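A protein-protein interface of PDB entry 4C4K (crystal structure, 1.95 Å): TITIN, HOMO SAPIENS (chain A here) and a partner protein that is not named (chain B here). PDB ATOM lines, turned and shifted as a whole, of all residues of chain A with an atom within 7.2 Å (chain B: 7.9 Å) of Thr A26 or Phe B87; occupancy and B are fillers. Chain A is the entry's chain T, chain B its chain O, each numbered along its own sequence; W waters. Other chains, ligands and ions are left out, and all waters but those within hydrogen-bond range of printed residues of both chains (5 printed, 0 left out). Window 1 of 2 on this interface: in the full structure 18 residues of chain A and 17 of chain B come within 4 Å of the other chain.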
ATOM      1  N   LEU A  13      17.121   8.668  30.663  1.00  0.00           N
ATOM      2  CA  LEU A  13      15.913   8.766  31.455  1.00  0.00           C
ATOM      3  C   LEU A  13      15.483  10.231  31.409  1.00  0.00           C
ATOM      4  O   LEU A  13      16.327  11.107  31.637  1.00  0.00           O
ATOM      5  CB  LEU A  13      16.138   8.285  32.914  1.00  0.00           C
ATOM      6  CG  LEU A  13      14.880   8.193  33.802  1.00  0.00           C
ATOM      7  CD1 LEU A  13      13.937   7.095  33.320  1.00  0.00           C
ATOM      8  CD2 LEU A  13      15.256   7.902  35.266  1.00  0.00           C
ATOM      9  N   PRO A  14      14.205  10.546  31.099  1.00  0.00           N
ATOM     10  CA  PRO A  14      13.810  11.958  31.076  1.00  0.00           C
ATOM     11  C   PRO A  14      13.998  12.545  32.467  1.00  0.00           C
ATOM     12  O   PRO A  14      13.896  11.813  33.463  1.00  0.00           O
ATOM     13  CB  PRO A  14      12.307  11.906  30.708  1.00  0.00           C
ATOM     14  CG  PRO A  14      12.078  10.584  30.109  1.00  0.00           C
ATOM     15  CD  PRO A  14      13.057   9.662  30.784  1.00  0.00           C
ATOM     16  N   ASP A  16      12.022  14.977  33.581  1.00  0.00           N
ATOM     17  CA  ASP A  16      10.672  15.384  33.970  1.00  0.00           C
ATOM     18  C   ASP A  16       9.658  14.838  33.022  1.00  0.00           C
ATOM     19  O   ASP A  16       9.839  14.879  31.795  1.00  0.00           O
ATOM     20  CB  ASP A  16      10.546  16.931  33.933  1.00  0.00           C
ATOM     21  CG  ASP A  16      11.420  17.641  34.947  1.00  0.00           C
ATOM     22  OD1 ASP A  16      12.580  17.926  34.626  1.00  0.00           O
ATOM     23  OD2 ASP A  16      10.956  17.850  36.086  1.00  0.00           O
ATOM     24  N   ILE A  17       8.560  14.353  33.581  1.00  0.00           N
ATOM     25  CA  ILE A  17       7.432  13.866  32.801  1.00  0.00           C
ATOM     26  C   ILE A  17       6.170  14.277  33.538  1.00  0.00           C
ATOM     27  O   ILE A  17       6.129  14.238  34.773  1.00  0.00           O
ATOM     28  CB  ILE A  17       7.489  12.329  32.494  1.00  0.00           C
ATOM     29  CG1 ILE A  17       7.428  11.468  33.754  1.00  0.00           C
ATOM     30  CG2 ILE A  17       8.684  11.949  31.621  1.00  0.00           C
ATOM     31  CD1 ILE A  17       7.726   9.949  33.483  1.00  0.00           C
ATOM     32  N   SER A  18       5.157  14.696  32.782  1.00  0.00           N
ATOM     33  CA  SER A  18       3.852  15.097  33.299  1.00  0.00           C
ATOM     34  C   SER A  18       2.777  14.104  32.882  1.00  0.00           C
ATOM     35  O   SER A  18       2.874  13.484  31.829  1.00  0.00           O
ATOM     36  CB  SER A  18       3.482  16.497  32.816  1.00  0.00           C
ATOM     37  OG  SER A  18       4.278  17.445  33.501  1.00  0.00           O
ATOM     38  N   ILE A  19       1.762  13.938  33.711  1.00  0.00           N
ATOM     39  CA  ILE A  19       0.665  13.013  33.412  1.00  0.00           C
ATOM     40  C   ILE A  19      -0.582  13.500  34.121  1.00  0.00           C
ATOM     41  O   ILE A  19      -0.500  13.986  35.249  1.00  0.00           O
ATOM     42  CB  ILE A  19       1.048  11.524  33.803  1.00  0.00           C
ATOM     43  CG1 ILE A  19      -0.034  10.478  33.373  1.00  0.00           C
ATOM     44  CG2 ILE A  19       1.405  11.367  35.279  1.00  0.00           C
ATOM     45  CD1 ILE A  19       0.008  10.035  31.907  1.00  0.00           C
ATOM     46  N   VAL A  24      -2.914   5.941  33.073  1.00  0.00           N
ATOM     47  CA  VAL A  24      -1.860   4.978  33.269  1.00  0.00           C
ATOM     48  C   VAL A  24      -0.589   5.646  32.753  1.00  0.00           C
ATOM     49  O   VAL A  24      -0.580   6.203  31.656  1.00  0.00           O
ATOM     50  CB  VAL A  24      -2.092   3.649  32.496  1.00  0.00           C
ATOM     51  CG1 VAL A  24      -0.872   2.712  32.598  1.00  0.00           C
ATOM     52  CG2 VAL A  24      -3.363   2.935  32.946  1.00  0.00           C
ATOM     53  N   LEU A  25       0.480   5.567  33.529  1.00  0.00           N
ATOM     54  CA  LEU A  25       1.752   6.108  33.114  1.00  0.00           C
ATOM     55  C   LEU A  25       2.770   4.959  33.038  1.00  0.00           C
ATOM     56  O   LEU A  25       2.837   4.124  33.952  1.00  0.00           O
ATOM     57  CB  LEU A  25       2.177   7.194  34.132  1.00  0.00           C
ATOM     58  CG  LEU A  25       3.522   7.957  33.998  1.00  0.00           C
ATOM     59  CD1 LEU A  25       4.636   7.269  34.752  1.00  0.00           C
ATOM     60  CD2 LEU A  25       3.880   8.333  32.552  1.00  0.00           C
ATOM     61  N   THR A  26       3.567   4.925  31.955  1.00  0.00           N
ATOM     62  CA  THR A  26       4.650   3.952  31.837  1.00  0.00           C
ATOM     63  C   THR A  26       5.897   4.696  31.432  1.00  0.00           C
ATOM     64  O   THR A  26       5.841   5.564  30.560  1.00  0.00           O
ATOM     65  CB  THR A  26       4.340   2.722  30.948  1.00  0.00           C
ATOM     66  OG1 THR A  26       4.355   3.118  29.599  1.00  0.00           O
ATOM     67  CG2 THR A  26       2.993   2.068  31.265  1.00  0.00           C
ATOM     68  N   VAL A  27       7.023   4.395  32.098  1.00  0.00           N
ATOM     69  CA  VAL A  27       8.319   4.988  31.782  1.00  0.00           C
ATOM     70  C   VAL A  27       9.259   3.805  31.528  1.00  0.00           C
ATOM     71  O   VAL A  27       9.488   3.005  32.432  1.00  0.00           O
ATOM     72  CB  VAL A  27       8.849   5.862  32.932  1.00  0.00           C
ATOM     73  CG1 VAL A  27      10.176   6.530  32.560  1.00  0.00           C
ATOM     74  CG2 VAL A  27       7.821   6.909  33.321  1.00  0.00           C
ATOM     75  N   ALA A  28       9.817   3.720  30.318  1.00  0.00           N
ATOM     76  CA  ALA A  28      10.723   2.627  29.981  1.00  0.00           C
ATOM     77  C   ALA A  28      12.137   3.165  29.841  1.00  0.00           C
ATOM     78  O   ALA A  28      12.342   4.284  29.363  1.00  0.00           O
ATOM     79  CB  ALA A  28      10.262   1.934  28.712  1.00  0.00           C
ATOM     80  N   CYS A  29      13.110   2.397  30.324  1.00  0.00           N
ATOM     81  CA  CYS A  29      14.511   2.808  30.306  1.00  0.00           C
ATOM     82  C   CYS A  29      15.445   1.647  29.954  1.00  0.00           C
ATOM     83  O   CYS A  29      15.413   0.608  30.601  1.00  0.00           O
ATOM     84  CB  CYS A  29      14.888   3.455  31.642  1.00  0.00           C
ATOM     85  SG  CYS A  29      16.530   4.219  31.645  1.00  0.00           S
ATOM     86  N   THR A  66      10.835  -1.223  33.035  1.00  0.00           N
ATOM     87  CA  THR A  66       9.664  -0.373  32.885  1.00  0.00           C
ATOM     88  C   THR A  66       8.986  -0.141  34.231  1.00  0.00           C
ATOM     89  O   THR A  66       8.672  -1.108  34.925  1.00  0.00           O
ATOM     90  CB  THR A  66       8.681  -0.986  31.863  1.00  0.00           C
ATOM     91  OG1 THR A  66       9.386  -1.269  30.643  1.00  0.00           O
ATOM     92  CG2 THR A  66       7.478  -0.068  31.582  1.00  0.00           C
ATOM     93  N   LEU A  67       8.729   1.140  34.571  1.00  0.00           N
ATOM     94  CA  LEU A  67       7.950   1.543  35.736  1.00  0.00           C
ATOM     95  C   LEU A  67       6.515   1.843  35.229  1.00  0.00           C
ATOM     96  O   LEU A  67       6.343   2.616  34.286  1.00  0.00           O
ATOM     97  CB  LEU A  67       8.545   2.824  36.388  1.00  0.00           C
ATOM     98  CG  LEU A  67       7.769   3.385  37.588  1.00  0.00           C
ATOM     99  CD1 LEU A  67       7.772   2.399  38.771  1.00  0.00           C
ATOM    100  CD2 LEU A  67       8.359   4.721  38.029  1.00  0.00           C
ATOM    101  N   ILE A  68       5.509   1.186  35.827  1.00  0.00           N
ATOM    102  CA  ILE A  68       4.099   1.363  35.468  1.00  0.00           C
ATOM    103  C   ILE A  68       3.366   1.860  36.677  1.00  0.00           C
ATOM    104  O   ILE A  68       3.491   1.287  37.750  1.00  0.00           O
ATOM    105  CB  ILE A  68       3.457   0.047  34.926  1.00  0.00           C
ATOM    106  CG1 ILE A  68       4.138  -0.415  33.614  1.00  0.00           C
ATOM    107  CG2 ILE A  68       1.931   0.186  34.729  1.00  0.00           C
ATOM    108  CD1 ILE A  68       4.187  -1.927  33.453  1.00  0.00           C
ATOM    109  N   ILE A  69       2.618   2.942  36.509  1.00  0.00           N
ATOM    110  CA  ILE A  69       1.748   3.457  37.545  1.00  0.00           C
ATOM    111  C   ILE A  69       0.360   3.511  36.911  1.00  0.00           C
ATOM    112  O   ILE A  69       0.105   4.343  36.045  1.00  0.00           O
ATOM    113  CB  ILE A  69       2.170   4.821  38.117  1.00  0.00           C
ATOM    114  CG1 ILE A  69       3.694   4.842  38.504  1.00  0.00           C
ATOM    115  CG2 ILE A  69       1.224   5.155  39.328  1.00  0.00           C
ATOM    116  CD1 ILE A  69       4.305   6.273  38.756  1.00  0.00           C
ATOM    117  N   MET A  70      -0.507   2.606  37.314  1.00  0.00           N
ATOM    118  CA  MET A  70      -1.891   2.569  36.851  1.00  0.00           C
ATOM    119  C   MET A  70      -2.719   3.486  37.689  1.00  0.00           C
ATOM    120  O   MET A  70      -2.430   3.639  38.880  1.00  0.00           O
ATOM    121  CB  MET A  70      -2.436   1.144  36.899  1.00  0.00           C
ATOM    122  CG  MET A  70      -1.704   0.239  35.924  1.00  0.00           C
ATOM    123  SD  MET A  70      -2.587  -1.267  35.549  1.00  0.00           S
ATOM    124  CE  MET A  70      -2.512  -2.106  37.140  1.00  0.00           C
ATOM    125  N   VAL A  72      -3.165   6.820  37.998  1.00  0.00           N
ATOM    126  CA  VAL A  72      -2.317   7.836  38.608  1.00  0.00           C
ATOM    127  C   VAL A  72      -3.096   8.743  39.569  1.00  0.00           C
ATOM    128  O   VAL A  72      -4.165   9.222  39.222  1.00  0.00           O
ATOM    129  CB  VAL A  72      -1.558   8.613  37.500  1.00  0.00           C
ATOM    130  CG1 VAL A  72      -1.061   9.960  37.992  1.00  0.00           C
ATOM    131  CG2 VAL A  72      -0.413   7.783  36.932  1.00  0.00           C
ATOM    132  N   ARG A 100      -0.970  16.282  36.688  1.00  0.00           N
ATOM    133  CA  ARG A 100      -1.883  17.370  36.313  1.00  0.00           C
ATOM    134  C   ARG A 100      -3.267  17.024  36.847  1.00  0.00           C
ATOM    135  O   ARG A 100      -3.782  15.918  36.598  1.00  0.00           O
ATOM    136  CB  ARG A 100      -1.966  17.537  34.777  1.00  0.00           C
ATOM    137  CG  ARG A 100      -0.661  17.896  34.070  1.00  0.00           C
ATOM    138  CD  ARG A 100      -0.971  18.271  32.628  1.00  0.00           C
ATOM    139  NE  ARG A 100       0.127  17.968  31.708  1.00  0.00           N
ATOM    140  CZ  ARG A 100       0.223  16.856  30.983  1.00  0.00           C
ATOM    141  NH1 ARG A 100      -0.706  15.915  31.072  1.00  0.00           N
ATOM    142  NH2 ARG A 100       1.247  16.680  30.161  1.00  0.00           N
ATOM    143  N   ALA B   4      -3.526   0.734  27.784  1.00  0.00           N
ATOM    144  CA  ALA B   4      -2.547   1.817  27.832  1.00  0.00           C
ATOM    145  C   ALA B   4      -1.340   1.511  26.933  1.00  0.00           C
ATOM    146  O   ALA B   4      -0.975   0.342  26.814  1.00  0.00           O
ATOM    147  CB  ALA B   4      -2.072   2.039  29.267  1.00  0.00           C
ATOM    148  N   PRO B   5      -0.668   2.537  26.364  1.00  0.00           N
ATOM    149  CA  PRO B   5       0.460   2.262  25.482  1.00  0.00           C
ATOM    150  C   PRO B   5       1.618   1.585  26.160  1.00  0.00           C
ATOM    151  O   PRO B   5       1.822   1.764  27.364  1.00  0.00           O
ATOM    152  CB  PRO B   5       0.848   3.645  24.931  1.00  0.00           C
ATOM    153  CG  PRO B   5      -0.361   4.495  25.133  1.00  0.00           C
ATOM    154  CD  PRO B   5      -0.954   3.987  26.416  1.00  0.00           C
ATOM    155  N   ARG B   6       2.355   0.785  25.375  1.00  0.00           N
ATOM    156  CA  ARG B   6       3.517   0.051  25.849  1.00  0.00           C
ATOM    157  C   ARG B   6       4.605  -0.006  24.788  1.00  0.00           C
ATOM    158  O   ARG B   6       4.314  -0.249  23.629  1.00  0.00           O
ATOM    159  CB  ARG B   6       3.092  -1.396  26.245  1.00  0.00           C
ATOM    160  CG  ARG B   6       4.253  -2.223  26.796  1.00  0.00           C
ATOM    161  CD  ARG B   6       4.148  -3.714  26.547  1.00  0.00           C
ATOM    162  NE  ARG B   6       3.378  -4.400  27.589  1.00  0.00           N
ATOM    163  CZ  ARG B   6       3.782  -4.566  28.844  1.00  0.00           C
ATOM    164  NH1 ARG B   6       4.951  -4.077  29.243  1.00  0.00           N
ATOM    165  NH2 ARG B   6       3.019  -5.212  29.712  1.00  0.00           N
ATOM    166  N   PHE B   7       5.859   0.193  25.197  1.00  0.00           N
ATOM    167  CA  PHE B   7       7.021   0.008  24.337  1.00  0.00           C
ATOM    168  C   PHE B   7       7.364  -1.485  24.367  1.00  0.00           C
ATOM    169  O   PHE B   7       7.711  -2.012  25.428  1.00  0.00           O
ATOM    170  CB  PHE B   7       8.209   0.822  24.846  1.00  0.00           C
ATOM    171  CG  PHE B   7       8.109   2.300  24.579  1.00  0.00           C
ATOM    172  CD1 PHE B   7       8.611   2.845  23.409  1.00  0.00           C
ATOM    173  CD2 PHE B   7       7.535   3.155  25.516  1.00  0.00           C
ATOM    174  CE1 PHE B   7       8.551   4.222  23.179  1.00  0.00           C
ATOM    175  CE2 PHE B   7       7.451   4.532  25.273  1.00  0.00           C
ATOM    176  CZ  PHE B   7       7.934   5.053  24.097  1.00  0.00           C
ATOM    177  N   PRO B  11      13.810   2.031  22.876  1.00  0.00           N
ATOM    178  CA  PRO B  11      14.021   2.975  21.758  1.00  0.00           C
ATOM    179  C   PRO B  11      15.482   2.897  21.354  1.00  0.00           C
ATOM    180  O   PRO B  11      16.348   2.677  22.206  1.00  0.00           O
ATOM    181  CB  PRO B  11      13.669   4.340  22.351  1.00  0.00           C
ATOM    182  CG  PRO B  11      13.856   4.171  23.830  1.00  0.00           C
ATOM    183  CD  PRO B  11      13.576   2.739  24.155  1.00  0.00           C
ATOM    184  N   SER B  37       4.805  10.961  19.394  1.00  0.00           N
ATOM    185  CA  SER B  37       5.567  12.169  19.104  1.00  0.00           C
ATOM    186  C   SER B  37       6.956  12.080  19.753  1.00  0.00           C
ATOM    187  O   SER B  37       7.148  11.312  20.691  1.00  0.00           O
ATOM    188  CB  SER B  37       4.816  13.413  19.598  1.00  0.00           C
ATOM    189  OG  SER B  37       4.648  13.352  21.001  1.00  0.00           O
ATOM    190  N   GLU B  39      10.274  14.400  21.451  1.00  0.00           N
ATOM    191  CA  GLU B  39      10.616  15.667  22.087  1.00  0.00           C
ATOM    192  C   GLU B  39      12.100  15.732  22.356  1.00  0.00           C
ATOM    193  O   GLU B  39      12.704  14.729  22.706  1.00  0.00           O
ATOM    194  CB  GLU B  39       9.840  15.863  23.418  1.00  0.00           C
ATOM    195  CG  GLU B  39       8.352  16.091  23.211  1.00  0.00           C
ATOM    196  CD  GLU B  39       7.459  15.993  24.431  1.00  0.00           C
ATOM    197  OE1 GLU B  39       7.971  16.114  25.569  1.00  0.00           O
ATOM    198  OE2 GLU B  39       6.231  15.825  24.244  1.00  0.00           O
ATOM    199  N   VAL B  76      13.058  12.130  23.628  1.00  0.00           N
ATOM    200  CA  VAL B  76      12.068  11.364  24.382  1.00  0.00           C
ATOM    201  C   VAL B  76      10.973  10.952  23.400  1.00  0.00           C
ATOM    202  O   VAL B  76      10.496  11.789  22.626  1.00  0.00           O
ATOM    203  CB  VAL B  76      11.491  12.186  25.584  1.00  0.00           C
ATOM    204  CG1 VAL B  76      10.406  11.395  26.330  1.00  0.00           C
ATOM    205  CG2 VAL B  76      12.607  12.604  26.545  1.00  0.00           C
ATOM    206  N   CYS B  77      10.582   9.672  23.414  1.00  0.00           N
ATOM    207  CA  CYS B  77       9.458   9.228  22.614  1.00  0.00           C
ATOM    208  C   CYS B  77       8.247   9.154  23.525  1.00  0.00           C
ATOM    209  O   CYS B  77       8.330   8.566  24.608  1.00  0.00           O
ATOM    210  CB  CYS B  77       9.734   7.891  21.945  1.00  0.00           C
ATOM    211  SG  CYS B  77       8.428   7.389  20.804  1.00  0.00           S
ATOM    212  N   ARG B  78       7.138   9.798  23.118  1.00  0.00           N
ATOM    213  CA  ARG B  78       5.903   9.865  23.893  1.00  0.00           C
ATOM    214  C   ARG B  78       4.777   9.214  23.101  1.00  0.00           C
ATOM    215  O   ARG B  78       4.560   9.576  21.950  1.00  0.00           O
ATOM    216  CB  ARG B  78       5.588  11.338  24.259  1.00  0.00           C
ATOM    217  CG  ARG B  78       4.282  11.570  25.032  1.00  0.00           C
ATOM    218  CD  ARG B  78       4.033  13.060  25.239  1.00  0.00           C
ATOM    219  NE  ARG B  78       2.770  13.313  25.939  1.00  0.00           N
ATOM    220  CZ  ARG B  78       1.762  14.037  25.458  1.00  0.00           C
ATOM    221  NH1 ARG B  78       1.858  14.615  24.264  1.00  0.00           N
ATOM    222  NH2 ARG B  78       0.651  14.195  26.169  1.00  0.00           N
ATOM    223  N   ALA B  79       4.092   8.228  23.705  1.00  0.00           N
ATOM    224  CA  ALA B  79       2.971   7.539  23.064  1.00  0.00           C
ATOM    225  C   ALA B  79       1.758   7.763  23.944  1.00  0.00           C
ATOM    226  O   ALA B  79       1.822   7.523  25.148  1.00  0.00           O
ATOM    227  CB  ALA B  79       3.263   6.048  22.929  1.00  0.00           C
ATOM    228  N   ARG B  80       0.676   8.265  23.371  1.00  0.00           N
ATOM    229  CA  ARG B  80      -0.489   8.525  24.179  1.00  0.00           C
ATOM    230  C   ARG B  80      -1.826   8.094  23.549  1.00  0.00           C
ATOM    231  O   ARG B  80      -1.998   8.176  22.340  1.00  0.00           O
ATOM    232  CB  ARG B  80      -0.490  10.002  24.613  1.00  0.00           C
ATOM    233  CG  ARG B  80      -0.915  11.037  23.587  1.00  0.00           C
ATOM    234  CD  ARG B  80      -2.007  11.894  24.209  1.00  0.00           C
ATOM    235  NE  ARG B  80      -2.168  13.198  23.559  1.00  0.00           N
ATOM    236  CZ  ARG B  80      -2.960  13.430  22.514  1.00  0.00           C
ATOM    237  NH1 ARG B  80      -3.653  12.440  21.962  1.00  0.00           N
ATOM    238  NH2 ARG B  80      -3.056  14.651  22.007  1.00  0.00           N
ATOM    239  N   GLY B  84      -3.814   6.108  28.596  1.00  0.00           N
ATOM    240  CA  GLY B  84      -2.570   6.490  29.224  1.00  0.00           C
ATOM    241  C   GLY B  84      -1.463   6.914  28.310  1.00  0.00           C
ATOM    242  O   GLY B  84      -1.660   7.105  27.114  1.00  0.00           O
ATOM    243  N   GLU B  85      -0.290   7.072  28.893  1.00  0.00           N
ATOM    244  CA  GLU B  85       0.863   7.514  28.126  1.00  0.00           C
ATOM    245  C   GLU B  85       2.068   6.705  28.489  1.00  0.00           C
ATOM    246  O   GLU B  85       2.256   6.374  29.676  1.00  0.00           O
ATOM    247  CB  GLU B  85       1.146   9.014  28.385  1.00  0.00           C
ATOM    248  CG  GLU B  85      -0.018   9.934  28.060  1.00  0.00           C
ATOM    249  CD  GLU B  85       0.302  11.414  27.999  1.00  0.00           C
ATOM    250  OE1 GLU B  85       1.484  11.779  27.792  1.00  0.00           O
ATOM    251  OE2 GLU B  85      -0.638  12.213  28.198  1.00  0.00           O
ATOM    252  N   ALA B  86       2.947   6.493  27.497  1.00  0.00           N
ATOM    253  CA  ALA B  86       4.213   5.817  27.693  1.00  0.00           C
ATOM    254  C   ALA B  86       5.336   6.739  27.238  1.00  0.00           C
ATOM    255  O   ALA B  86       5.209   7.416  26.209  1.00  0.00           O
ATOM    256  CB  ALA B  86       4.242   4.501  26.910  1.00  0.00           C
ATOM    257  N   PHE B  87       6.443   6.772  28.012  1.00  0.00           N
ATOM    258  CA  PHE B  87       7.623   7.578  27.688  1.00  0.00           C
ATOM    259  C   PHE B  87       8.884   6.703  27.698  1.00  0.00           C
ATOM    260  O   PHE B  87       9.002   5.832  28.545  1.00  0.00           O
ATOM    261  CB  PHE B  87       7.806   8.702  28.727  1.00  0.00           C
ATOM    262  CG  PHE B  87       6.689   9.703  28.821  1.00  0.00           C
ATOM    263  CD1 PHE B  87       5.500   9.385  29.479  1.00  0.00           C
ATOM    264  CD2 PHE B  87       6.853  10.995  28.337  1.00  0.00           C
ATOM    265  CE1 PHE B  87       4.460  10.311  29.567  1.00  0.00           C
ATOM    266  CE2 PHE B  87       5.816  11.930  28.440  1.00  0.00           C
ATOM    267  CZ  PHE B  87       4.630  11.579  29.062  1.00  0.00           C
ATOM    268  N   ALA B  88       9.849   6.980  26.802  1.00  0.00           N
ATOM    269  CA  ALA B  88      11.143   6.290  26.734  1.00  0.00           C
ATOM    270  C   ALA B  88      12.094   7.214  26.022  1.00  0.00           C
ATOM    271  O   ALA B  88      11.738   7.786  25.002  1.00  0.00           O
ATOM    272  CB  ALA B  88      11.031   4.960  25.981  1.00  0.00           C
ATOM    273  N   ALA B  89      13.296   7.394  26.570  1.00  0.00           N
ATOM    274  CA  ALA B  89      14.255   8.309  25.990  1.00  0.00           C
ATOM    275  C   ALA B  89      15.433   7.571  25.398  1.00  0.00           C
ATOM    276  O   ALA B  89      15.659   6.402  25.698  1.00  0.00           O
ATOM    277  CB  ALA B  89      14.719   9.313  27.042  1.00  0.00           C
HETATM  278  O   HOH W   1       1.855  14.061  29.289  1.00  0.00           O
HETATM  279  O   HOH W   2      -1.964  13.026  30.449  1.00  0.00           O
HETATM  280  O   HOH W   3       7.611  -1.223  28.407  1.00  0.00           O
HETATM  281  O   HOH W   4      13.710   6.574  29.288  1.00  0.00           O
HETATM  282  O   HOH W   5       6.322   0.766  27.978  1.00  0.00           O
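Among the printed residues, pairs that only touch across the chains: Ile A17 with Phe B87 (3.9 Å), Ser A18 with Phe B87 (3.8 Å), Ile A19 with Glu B85 (3.8 Å), Val A24 with Ala B4 (3.6 Å), Val A24 with Gly B84 (3.2 Å), Leu A25 with Glu B85 (3.5 Å), Leu A25 with Phe B87 (3.6 Å), Thr A26 with Pro B5 (3.6 Å), Thr A26 with Ala B86 (3.0 Å), Val A27 with Phe B87 (3.4 Å) and Ala A28 with Ala B88 (3.5 Å).
Of the 18 printed residues of chain B, 7 touch a printed residue of chain A. Hydrophobic or aromatic side chains of chain B that line the printed part of chain A: Ala B4, Ala B86, Phe B87 and Ala B88. Among the printed residues, 15 pairs touch across the chains.
The backbone NH (N) of Leu A25 lies within hydrogen-bond range of the backbone carbonyl oxygen (O) of Ile A69 (2.8 Å). NE of Arg B78 lies within salt-bridge range of OE1 of Glu B85, at 2.7 Å. The backbone carbonyl oxygen (O) of Ile A19 sits at hydrogen-bond distance from the backbone NH (N) of Arg A100 (2.8 Å). N of Val A27 lies within hydrogen-bond range of O of Leu A67, at 2.9 Å. O of Ala B79 sits at hydrogen-bond distance from N of Ala B86. The backbone carbonyl oxygen (O) of Ala B88 sits at hydrogen-bond distance from the backbone NH (N) of Cys B77 (2.7 Å).
O of Phe B87 sits at hydrogen-bond distance from N of Ala A28. The backbone carbonyl oxygen of Glu B85 sits at hydrogen-bond distance from the backbone NH of Thr A26 (3.0 Å). O of Thr A26 lies within hydrogen-bond range of N of Phe B87. N of Glu B85 sits at hydrogen-bond distance from O of Val A24, 2.9 Å away.
Water W4 bridges the backbone carbonyl oxygen of Ala A28 and the backbone NH of Ala B89. Water W2 bridges the side-chain carboxylate of Glu B85 (2.7 Å) and the guanidinium group of Arg A100 (3.2 Å). Water W1 lies within hydrogen-bond range of OE1 of Glu B85, O of Ser A18, NH2 of Arg A100 and NH2 of Arg B78. Water W3 bridges OG1 of Thr A66 (2.9 Å) and O of Phe B7 (3.1 Å). Water W5 lies within hydrogen-bond range of N of Phe B7 (2.9 Å) and OG1 of Thr A26 (3.5 Å).
Thr A26 touches just these residues of chain B: Pro B5 (3.6 Å), Glu B85 (3.0 Å), Ala B86 (3.0 Å) and Phe B87 (2.9 Å). Of the printed residues of chain A, Phe B87 touches Ile A17, Ser A18, Leu A25, Thr A26, Val A27 and Ala A28. Of the printed residues of chain A, Gly B84 touches Val A24. Of the printed residues of chain B, Ser A18 touches Phe B87 (3.8 Å). Printed residues of chain B within 4 Å of Ile A17: Phe B87 (3.9 Å). Printed residues of chain A within 4 Å of Glu B85: Ile A19 (3.8 Å), Val A24 (2.9 Å), Leu A25 (3.5 Å) and Thr A26 (3.0 Å). Of the printed residues of chain A, Ala B88 touches Ala A28. Arg B6 touches none of the printed residues of chain A. Glu B39 touches none of the printed residues of chain A. The nearest residue of chain B that does not touch Thr A26 is Arg B6 (4.9 Å). The nearest printed residue of chain A that does not touch Phe B87 is Pro A14 (4.9 Å).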
